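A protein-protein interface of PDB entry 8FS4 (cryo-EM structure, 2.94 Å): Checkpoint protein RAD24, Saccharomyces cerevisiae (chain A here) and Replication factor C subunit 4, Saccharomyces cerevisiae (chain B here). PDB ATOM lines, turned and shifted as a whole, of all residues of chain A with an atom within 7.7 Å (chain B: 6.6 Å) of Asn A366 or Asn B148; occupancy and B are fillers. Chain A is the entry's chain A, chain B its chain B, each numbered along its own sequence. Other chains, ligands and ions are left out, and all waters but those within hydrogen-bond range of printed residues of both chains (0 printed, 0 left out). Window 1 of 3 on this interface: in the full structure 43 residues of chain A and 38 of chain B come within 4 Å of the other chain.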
ATOM      1  N   GLU A 227      -0.659 -15.901 -26.855  1.00  0.00           N
ATOM      2  CA  GLU A 227      -1.753 -15.819 -25.901  1.00  0.00           C
ATOM      3  C   GLU A 227      -1.721 -14.475 -25.192  1.00  0.00           C
ATOM      4  O   GLU A 227      -0.669 -14.027 -24.729  1.00  0.00           O
ATOM      5  CB  GLU A 227      -1.652 -16.956 -24.885  1.00  0.00           C
ATOM      6  CG  GLU A 227      -2.780 -16.966 -23.861  1.00  0.00           C
ATOM      7  CD  GLU A 227      -3.704 -18.159 -24.002  1.00  0.00           C
ATOM      8  OE1 GLU A 227      -4.896 -18.021 -23.645  1.00  0.00           O
ATOM      9  OE2 GLU A 227      -3.249 -19.226 -24.455  1.00  0.00           O
ATOM     10  N   ILE A 228      -2.878 -13.832 -25.113  1.00  0.00           N
ATOM     11  CA  ILE A 228      -2.999 -12.504 -24.523  1.00  0.00           C
ATOM     12  C   ILE A 228      -3.291 -12.677 -23.034  1.00  0.00           C
ATOM     13  O   ILE A 228      -4.294 -13.320 -22.687  1.00  0.00           O
ATOM     14  CB  ILE A 228      -4.094 -11.680 -25.207  1.00  0.00           C
ATOM     15  CG1 ILE A 228      -3.919 -11.717 -26.728  1.00  0.00           C
ATOM     16  CG2 ILE A 228      -4.056 -10.245 -24.720  1.00  0.00           C
ATOM     17  CD1 ILE A 228      -5.209 -11.590 -27.472  1.00  0.00           C
ATOM     18  N   PRO A 229      -2.460 -12.136 -22.137  1.00  0.00           N
ATOM     19  CA  PRO A 229      -2.652 -12.397 -20.703  1.00  0.00           C
ATOM     20  C   PRO A 229      -4.008 -11.974 -20.164  1.00  0.00           C
ATOM     21  O   PRO A 229      -4.809 -11.344 -20.860  1.00  0.00           O
ATOM     22  CB  PRO A 229      -1.532 -11.577 -20.057  1.00  0.00           C
ATOM     23  CG  PRO A 229      -0.477 -11.526 -21.090  1.00  0.00           C
ATOM     24  CD  PRO A 229      -1.205 -11.407 -22.389  1.00  0.00           C
ATOM     25  N   GLU A 230      -4.261 -12.327 -18.905  1.00  0.00           N
ATOM     26  CA  GLU A 230      -5.512 -11.994 -18.239  1.00  0.00           C
ATOM     27  C   GLU A 230      -5.557 -10.495 -17.965  1.00  0.00           C
ATOM     28  O   GLU A 230      -4.643  -9.944 -17.340  1.00  0.00           O
ATOM     29  CB  GLU A 230      -5.640 -12.790 -16.943  1.00  0.00           C
ATOM     30  CG  GLU A 230      -5.651 -14.295 -17.156  1.00  0.00           C
ATOM     31  CD  GLU A 230      -6.142 -15.057 -15.940  1.00  0.00           C
ATOM     32  OE1 GLU A 230      -6.125 -14.485 -14.831  1.00  0.00           O
ATOM     33  OE2 GLU A 230      -6.541 -16.230 -16.095  1.00  0.00           O
ATOM     34  N   GLU A 334       9.314 -17.075 -21.538  1.00  0.00           N
ATOM     35  CA  GLU A 334       8.400 -18.180 -21.285  1.00  0.00           C
ATOM     36  C   GLU A 334       7.342 -18.225 -22.379  1.00  0.00           C
ATOM     37  O   GLU A 334       6.759 -17.195 -22.729  1.00  0.00           O
ATOM     38  CB  GLU A 334       7.740 -18.034 -19.913  1.00  0.00           C
ATOM     39  CG  GLU A 334       7.975 -19.207 -18.970  1.00  0.00           C
ATOM     40  CD  GLU A 334       7.617 -20.552 -19.582  1.00  0.00           C
ATOM     41  OE1 GLU A 334       7.103 -20.582 -20.720  1.00  0.00           O
ATOM     42  OE2 GLU A 334       7.859 -21.585 -18.924  1.00  0.00           O
ATOM     43  N   SER A 335       7.105 -19.418 -22.915  1.00  0.00           N
ATOM     44  CA  SER A 335       6.112 -19.629 -23.957  1.00  0.00           C
ATOM     45  C   SER A 335       4.885 -20.325 -23.382  1.00  0.00           C
ATOM     46  O   SER A 335       4.961 -21.027 -22.371  1.00  0.00           O
ATOM     47  CB  SER A 335       6.691 -20.460 -25.104  1.00  0.00           C
ATOM     48  OG  SER A 335       5.700 -20.740 -26.075  1.00  0.00           O
ATOM     49  N   THR A 336       3.750 -20.123 -24.042  1.00  0.00           N
ATOM     50  CA  THR A 336       2.473 -20.661 -23.598  1.00  0.00           C
ATOM     51  C   THR A 336       2.177 -21.972 -24.312  1.00  0.00           C
ATOM     52  O   THR A 336       2.443 -22.116 -25.508  1.00  0.00           O
ATOM     53  CB  THR A 336       1.342 -19.666 -23.859  1.00  0.00           C
ATOM     54  OG1 THR A 336       1.584 -18.973 -25.090  1.00  0.00           O
ATOM     55  CG2 THR A 336       1.246 -18.660 -22.724  1.00  0.00           C
ATOM     56  N   ILE A 337       1.621 -22.927 -23.568  1.00  0.00           N
ATOM     57  CA  ILE A 337       1.259 -24.225 -24.128  1.00  0.00           C
ATOM     58  C   ILE A 337       0.017 -24.060 -24.994  1.00  0.00           C
ATOM     59  O   ILE A 337      -0.702 -23.060 -24.887  1.00  0.00           O
ATOM     60  CB  ILE A 337       1.038 -25.290 -23.032  1.00  0.00           C
ATOM     61  CG1 ILE A 337       0.258 -24.743 -21.830  1.00  0.00           C
ATOM     62  CG2 ILE A 337       2.370 -25.830 -22.546  1.00  0.00           C
ATOM     63  CD1 ILE A 337      -1.108 -24.189 -22.152  1.00  0.00           C
ATOM     64  N   ILE A 360       0.690 -29.722 -12.473  1.00  0.00           N
ATOM     65  CA  ILE A 360      -0.633 -29.104 -12.465  1.00  0.00           C
ATOM     66  C   ILE A 360      -0.546 -27.664 -11.974  1.00  0.00           C
ATOM     67  O   ILE A 360      -1.150 -26.753 -12.557  1.00  0.00           O
ATOM     68  CB  ILE A 360      -1.601 -29.935 -11.602  1.00  0.00           C
ATOM     69  CG1 ILE A 360      -2.103 -31.158 -12.377  1.00  0.00           C
ATOM     70  CG2 ILE A 360      -2.772 -29.085 -11.132  1.00  0.00           C
ATOM     71  CD1 ILE A 360      -3.034 -30.838 -13.535  1.00  0.00           C
ATOM     72  N   ASN A 361       0.199 -27.436 -10.888  1.00  0.00           N
ATOM     73  CA  ASN A 361       0.305 -26.089 -10.343  1.00  0.00           C
ATOM     74  C   ASN A 361       0.950 -25.143 -11.343  1.00  0.00           C
ATOM     75  O   ASN A 361       0.506 -24.002 -11.501  1.00  0.00           O
ATOM     76  CB  ASN A 361       1.098 -26.109  -9.037  1.00  0.00           C
ATOM     77  CG  ASN A 361       0.268 -26.567  -7.860  1.00  0.00           C
ATOM     78  OD1 ASN A 361      -0.951 -26.412  -7.849  1.00  0.00           O
ATOM     79  ND2 ASN A 361       0.926 -27.130  -6.856  1.00  0.00           N
ATOM     80  N   ASN A 362       2.005 -25.594 -12.023  1.00  0.00           N
ATOM     81  CA  ASN A 362       2.647 -24.745 -13.019  1.00  0.00           C
ATOM     82  C   ASN A 362       1.710 -24.463 -14.185  1.00  0.00           C
ATOM     83  O   ASN A 362       1.672 -23.339 -14.703  1.00  0.00           O
ATOM     84  CB  ASN A 362       3.934 -25.399 -13.513  1.00  0.00           C
ATOM     85  CG  ASN A 362       5.004 -25.451 -12.444  1.00  0.00           C
ATOM     86  OD1 ASN A 362       4.781 -25.043 -11.305  1.00  0.00           O
ATOM     87  ND2 ASN A 362       6.177 -25.952 -12.806  1.00  0.00           N
ATOM     88  N   LEU A 363       0.943 -25.467 -14.613  1.00  0.00           N
ATOM     89  CA  LEU A 363       0.003 -25.251 -15.705  1.00  0.00           C
ATOM     90  C   LEU A 363      -1.043 -24.213 -15.324  1.00  0.00           C
ATOM     91  O   LEU A 363      -1.430 -23.380 -16.152  1.00  0.00           O
ATOM     92  CB  LEU A 363      -0.662 -26.571 -16.096  1.00  0.00           C
ATOM     93  CG  LEU A 363      -1.184 -26.667 -17.532  1.00  0.00           C
ATOM     94  CD1 LEU A 363      -0.044 -26.585 -18.528  1.00  0.00           C
ATOM     95  CD2 LEU A 363      -1.965 -27.953 -17.735  1.00  0.00           C
ATOM     96  N   PHE A 364      -1.516 -24.248 -14.078  1.00  0.00           N
ATOM     97  CA  PHE A 364      -2.481 -23.243 -13.640  1.00  0.00           C
ATOM     98  C   PHE A 364      -1.838 -21.868 -13.522  1.00  0.00           C
ATOM     99  O   PHE A 364      -2.440 -20.861 -13.912  1.00  0.00           O
ATOM    100  CB  PHE A 364      -3.104 -23.655 -12.308  1.00  0.00           C
ATOM    101  CG  PHE A 364      -4.282 -24.570 -12.450  1.00  0.00           C
ATOM    102  CD1 PHE A 364      -5.336 -24.244 -13.285  1.00  0.00           C
ATOM    103  CD2 PHE A 364      -4.329 -25.763 -11.758  1.00  0.00           C
ATOM    104  CE1 PHE A 364      -6.412 -25.085 -13.419  1.00  0.00           C
ATOM    105  CE2 PHE A 364      -5.400 -26.612 -11.894  1.00  0.00           C
ATOM    106  CZ  PHE A 364      -6.446 -26.271 -12.722  1.00  0.00           C
ATOM    107  N   GLU A 365      -0.618 -21.802 -12.986  1.00  0.00           N
ATOM    108  CA  GLU A 365       0.046 -20.515 -12.809  1.00  0.00           C
ATOM    109  C   GLU A 365       0.284 -19.835 -14.151  1.00  0.00           C
ATOM    110  O   GLU A 365      -0.127 -18.689 -14.361  1.00  0.00           O
ATOM    111  CB  GLU A 365       1.366 -20.718 -12.056  1.00  0.00           C
ATOM    112  CG  GLU A 365       2.474 -19.689 -12.331  1.00  0.00           C
ATOM    113  CD  GLU A 365       3.858 -20.235 -12.046  1.00  0.00           C
ATOM    114  OE1 GLU A 365       4.647 -19.538 -11.376  1.00  0.00           O
ATOM    115  OE2 GLU A 365       4.163 -21.357 -12.501  1.00  0.00           O
ATOM    116  N   ASN A 366       0.941 -20.533 -15.077  1.00  0.00           N
ATOM    117  CA  ASN A 366       1.311 -19.909 -16.341  1.00  0.00           C
ATOM    118  C   ASN A 366       0.158 -19.898 -17.331  1.00  0.00           C
ATOM    119  O   ASN A 366       0.071 -18.987 -18.162  1.00  0.00           O
ATOM    120  CB  ASN A 366       2.512 -20.631 -16.954  1.00  0.00           C
ATOM    121  CG  ASN A 366       3.837 -20.250 -16.303  1.00  0.00           C
ATOM    122  OD1 ASN A 366       3.984 -19.132 -15.812  1.00  0.00           O
ATOM    123  ND2 ASN A 366       4.795 -21.174 -16.275  1.00  0.00           N
ATOM    124  N   SER A 367      -0.730 -20.890 -17.264  1.00  0.00           N
ATOM    125  CA  SER A 367      -1.866 -21.000 -18.179  1.00  0.00           C
ATOM    126  C   SER A 367      -3.133 -21.117 -17.340  1.00  0.00           C
ATOM    127  O   SER A 367      -3.593 -22.216 -17.030  1.00  0.00           O
ATOM    128  CB  SER A 367      -1.693 -22.184 -19.117  1.00  0.00           C
ATOM    129  OG  SER A 367      -0.385 -22.204 -19.660  1.00  0.00           O
ATOM    130  N   ASN A 368      -3.687 -19.967 -16.961  1.00  0.00           N
ATOM    131  CA  ASN A 368      -5.016 -19.889 -16.371  1.00  0.00           C
ATOM    132  C   ASN A 368      -5.985 -19.150 -17.281  1.00  0.00           C
ATOM    133  O   ASN A 368      -7.136 -18.924 -16.897  1.00  0.00           O
ATOM    134  CB  ASN A 368      -4.953 -19.214 -15.000  1.00  0.00           C
ATOM    135  CG  ASN A 368      -5.720 -19.977 -13.939  1.00  0.00           C
ATOM    136  OD1 ASN A 368      -6.523 -20.856 -14.248  1.00  0.00           O
ATOM    137  ND2 ASN A 368      -5.469 -19.648 -12.679  1.00  0.00           N
ATOM    138  N   ASN A 369      -5.539 -18.765 -18.474  1.00  0.00           N
ATOM    139  CA  ASN A 369      -6.398 -18.167 -19.482  1.00  0.00           C
ATOM    140  C   ASN A 369      -7.058 -19.209 -20.373  1.00  0.00           C
ATOM    141  O   ASN A 369      -7.934 -18.857 -21.170  1.00  0.00           O
ATOM    142  CB  ASN A 369      -5.582 -17.196 -20.341  1.00  0.00           C
ATOM    143  CG  ASN A 369      -6.423 -16.084 -20.924  1.00  0.00           C
ATOM    144  OD1 ASN A 369      -7.430 -15.678 -20.345  1.00  0.00           O
ATOM    145  ND2 ASN A 369      -6.007 -15.575 -22.076  1.00  0.00           N
ATOM    146  N   LEU A 370      -6.655 -20.469 -20.256  1.00  0.00           N
ATOM    147  CA  LEU A 370      -7.275 -21.593 -20.945  1.00  0.00           C
ATOM    148  C   LEU A 370      -7.821 -22.628 -19.982  1.00  0.00           C
ATOM    149  O   LEU A 370      -8.901 -23.174 -20.213  1.00  0.00           O
ATOM    150  CB  LEU A 370      -6.262 -22.264 -21.881  1.00  0.00           C
ATOM    151  CG  LEU A 370      -6.457 -22.000 -23.370  1.00  0.00           C
ATOM    152  CD1 LEU A 370      -6.258 -20.532 -23.664  1.00  0.00           C
ATOM    153  CD2 LEU A 370      -5.490 -22.839 -24.176  1.00  0.00           C
ATOM    154  N   LEU A 371      -7.100 -22.904 -18.898  1.00  0.00           N
ATOM    155  CA  LEU A 371      -7.585 -23.817 -17.877  1.00  0.00           C
ATOM    156  C   LEU A 371      -8.777 -23.253 -17.117  1.00  0.00           C
ATOM    157  O   LEU A 371      -9.348 -23.960 -16.281  1.00  0.00           O
ATOM    158  CB  LEU A 371      -6.452 -24.147 -16.907  1.00  0.00           C
ATOM    159  CG  LEU A 371      -5.559 -25.309 -17.342  1.00  0.00           C
ATOM    160  CD1 LEU A 371      -4.687 -24.915 -18.521  1.00  0.00           C
ATOM    161  CD2 LEU A 371      -4.707 -25.779 -16.183  1.00  0.00           C
ATOM    162  N   CYS B 144       7.645  -5.772 -13.101  1.00  0.00           N
ATOM    163  CA  CYS B 144       6.349  -6.396 -12.897  1.00  0.00           C
ATOM    164  C   CYS B 144       6.450  -7.393 -11.755  1.00  0.00           C
ATOM    165  O   CYS B 144       7.533  -7.675 -11.240  1.00  0.00           O
ATOM    166  CB  CYS B 144       5.863  -7.088 -14.172  1.00  0.00           C
ATOM    167  SG  CYS B 144       7.056  -8.241 -14.866  1.00  0.00           S
ATOM    168  N   GLN B 146       4.403 -10.429 -12.137  1.00  0.00           N
ATOM    169  CA  GLN B 146       4.212 -11.683 -12.856  1.00  0.00           C
ATOM    170  C   GLN B 146       4.599 -11.458 -14.308  1.00  0.00           C
ATOM    171  O   GLN B 146       3.950 -10.677 -15.011  1.00  0.00           O
ATOM    172  CB  GLN B 146       2.763 -12.167 -12.747  1.00  0.00           C
ATOM    173  CG  GLN B 146       2.194 -12.077 -11.342  1.00  0.00           C
ATOM    174  CD  GLN B 146       0.834 -12.730 -11.224  1.00  0.00           C
ATOM    175  OE1 GLN B 146       0.590 -13.789 -11.802  1.00  0.00           O
ATOM    176  NE2 GLN B 146      -0.063 -12.099 -10.475  1.00  0.00           N
ATOM    177  N   SER B 147       5.653 -12.141 -14.755  1.00  0.00           N
ATOM    178  CA  SER B 147       6.202 -11.882 -16.081  1.00  0.00           C
ATOM    179  C   SER B 147       5.281 -12.335 -17.202  1.00  0.00           C
ATOM    180  O   SER B 147       5.439 -11.873 -18.336  1.00  0.00           O
ATOM    181  CB  SER B 147       7.557 -12.571 -16.230  1.00  0.00           C
ATOM    182  OG  SER B 147       8.117 -12.306 -17.503  1.00  0.00           O
ATOM    183  N   ASN B 148       4.327 -13.225 -16.922  1.00  0.00           N
ATOM    184  CA  ASN B 148       3.461 -13.727 -17.981  1.00  0.00           C
ATOM    185  C   ASN B 148       2.479 -12.673 -18.470  1.00  0.00           C
ATOM    186  O   ASN B 148       1.919 -12.827 -19.560  1.00  0.00           O
ATOM    187  CB  ASN B 148       2.694 -14.960 -17.507  1.00  0.00           C
ATOM    188  CG  ASN B 148       3.514 -15.839 -16.588  1.00  0.00           C
ATOM    189  OD1 ASN B 148       3.125 -16.104 -15.452  1.00  0.00           O
ATOM    190  ND2 ASN B 148       4.665 -16.289 -17.074  1.00  0.00           N
ATOM    191  N   LYS B 149       2.263 -11.608 -17.699  1.00  0.00           N
ATOM    192  CA  LYS B 149       1.329 -10.570 -18.107  1.00  0.00           C
ATOM    193  C   LYS B 149       1.889  -9.678 -19.204  1.00  0.00           C
ATOM    194  O   LYS B 149       1.138  -8.874 -19.765  1.00  0.00           O
ATOM    195  CB  LYS B 149       0.926  -9.713 -16.907  1.00  0.00           C
ATOM    196  CG  LYS B 149       0.590 -10.501 -15.644  1.00  0.00           C
ATOM    197  CD  LYS B 149      -0.828 -11.056 -15.678  1.00  0.00           C
ATOM    198  CE  LYS B 149      -1.629 -10.643 -14.451  1.00  0.00           C
ATOM    199  NZ  LYS B 149      -0.905 -10.892 -13.171  1.00  0.00           N
ATOM    200  N   ILE B 150       3.175  -9.790 -19.514  1.00  0.00           N
ATOM    201  CA  ILE B 150       3.769  -9.076 -20.637  1.00  0.00           C
ATOM    202  C   ILE B 150       3.775 -10.009 -21.839  1.00  0.00           C
ATOM    203  O   ILE B 150       4.209 -11.162 -21.739  1.00  0.00           O
ATOM    204  CB  ILE B 150       5.188  -8.589 -20.297  1.00  0.00           C
ATOM    205  CG1 ILE B 150       5.160  -7.685 -19.064  1.00  0.00           C
ATOM    206  CG2 ILE B 150       5.788  -7.824 -21.466  1.00  0.00           C
ATOM    207  CD1 ILE B 150       6.403  -7.768 -18.230  1.00  0.00           C
ATOM    208  N   ILE B 151       3.286  -9.512 -22.977  1.00  0.00           N
ATOM    209  CA  ILE B 151       3.091 -10.374 -24.131  1.00  0.00           C
ATOM    210  C   ILE B 151       4.426 -10.946 -24.593  1.00  0.00           C
ATOM    211  O   ILE B 151       5.484 -10.321 -24.452  1.00  0.00           O
ATOM    212  CB  ILE B 151       2.393  -9.609 -25.268  1.00  0.00           C
ATOM    213  CG1 ILE B 151       3.244  -8.424 -25.726  1.00  0.00           C
ATOM    214  CG2 ILE B 151       1.031  -9.130 -24.811  1.00  0.00           C
ATOM    215  CD1 ILE B 151       2.755  -7.785 -27.005  1.00  0.00           C
ATOM    216  N   GLU B 152       4.372 -12.154 -25.153  1.00  0.00           N
ATOM    217  CA  GLU B 152       5.596 -12.832 -25.566  1.00  0.00           C
ATOM    218  C   GLU B 152       6.424 -12.023 -26.555  1.00  0.00           C
ATOM    219  O   GLU B 152       7.661 -12.069 -26.460  1.00  0.00           O
ATOM    220  CB  GLU B 152       5.253 -14.208 -26.146  1.00  0.00           C
ATOM    221  CG  GLU B 152       4.668 -15.171 -25.127  1.00  0.00           C
ATOM    222  CD  GLU B 152       4.044 -16.392 -25.771  1.00  0.00           C
ATOM    223  OE1 GLU B 152       4.464 -16.757 -26.889  1.00  0.00           O
ATOM    224  OE2 GLU B 152       3.132 -16.988 -25.160  1.00  0.00           O
ATOM    225  N   GLN B 155       8.536  -9.823 -24.398  1.00  0.00           N
ATOM    226  CA  GLN B 155       9.537 -10.589 -23.668  1.00  0.00           C
ATOM    227  C   GLN B 155      10.635 -11.109 -24.581  1.00  0.00           C
ATOM    228  O   GLN B 155      11.735 -11.406 -24.105  1.00  0.00           O
ATOM    229  CB  GLN B 155       8.883 -11.765 -22.946  1.00  0.00           C
ATOM    230  CG  GLN B 155       7.723 -11.381 -22.058  1.00  0.00           C
ATOM    231  CD  GLN B 155       7.346 -12.482 -21.093  1.00  0.00           C
ATOM    232  OE1 GLN B 155       8.193 -13.009 -20.373  1.00  0.00           O
ATOM    233  NE2 GLN B 155       6.069 -12.839 -21.073  1.00  0.00           N
ATOM    234  N   ARG B 162      14.844 -12.465 -13.086  1.00  0.00           N
ATOM    235  CA  ARG B 162      13.875 -12.853 -12.072  1.00  0.00           C
ATOM    236  C   ARG B 162      14.494 -12.667 -10.694  1.00  0.00           C
ATOM    237  O   ARG B 162      15.547 -13.242 -10.398  1.00  0.00           O
ATOM    238  CB  ARG B 162      13.431 -14.299 -12.279  1.00  0.00           C
ATOM    239  CG  ARG B 162      12.838 -14.560 -13.654  1.00  0.00           C
ATOM    240  CD  ARG B 162      12.280 -15.967 -13.767  1.00  0.00           C
ATOM    241  NE  ARG B 162      12.304 -16.451 -15.143  1.00  0.00           N
ATOM    242  CZ  ARG B 162      11.362 -16.208 -16.045  1.00  0.00           C
ATOM    243  NH1 ARG B 162      10.295 -15.483 -15.753  1.00  0.00           N
ATOM    244  NH2 ARG B 162      11.495 -16.704 -17.271  1.00  0.00           N
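OE2 of Glu B152 is in hydrogen-bond range of OG1 of Thr A336, 2.5 Å away. OD1 of Asn B148 sits close to OD1 of Asn A366, 3.2 Å away.
Printed residues of chain B within 4 Å of Glu A334: Glu B152. Asn A361 touches none of the printed residues of chain B. Cys B144 touches none of the printed residues of chain A. Of the printed residues of chain A, Asn B148 touches Pro A229 and Asn A366. Printed residues of chain A within 4 Å of Glu B152: Glu A334 and Thr A336. The nearest printed residue of chain B that does not touch Asn A366 is Ser B147 (7.1 Å). The nearest residue of chain A that does not touch Asn B148 is Glu A365 (4.3 Å). The nearest printed residue of chain A that does not touch Lys B149 is Glu A230 (4.2 Å).
NE2 of Gln B146 sits close to NZ of Lys B149, 3.1 Å away.
Among the printed residues, merely in contact across the chains: Pro A229 with Asn B148 (3.1 Å), Pro A229 with Lys B149 (3.4 Å) and Glu A334 with Glu B152 (3.8 Å).
Of the 20 printed residues of chain A, 4 touch a printed residue of chain B. Printed residues of chain A that touch a printed residue of chain B: Pro A229, Glu A334, Thr A336 and Asn A366. Hydrophobic or aromatic side chains of chain A within 4 Å of the printed part of chain B: Pro A229. Of the 10 printed residues of chain B, 3 touch a printed residue of chain A. Among the printed residues, 5 pairs touch across the chains. Among the printed residues, no Asp or Glu carboxylate lies within 4 Å of a Lys or Arg side-chain nitrogen of the other chain.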
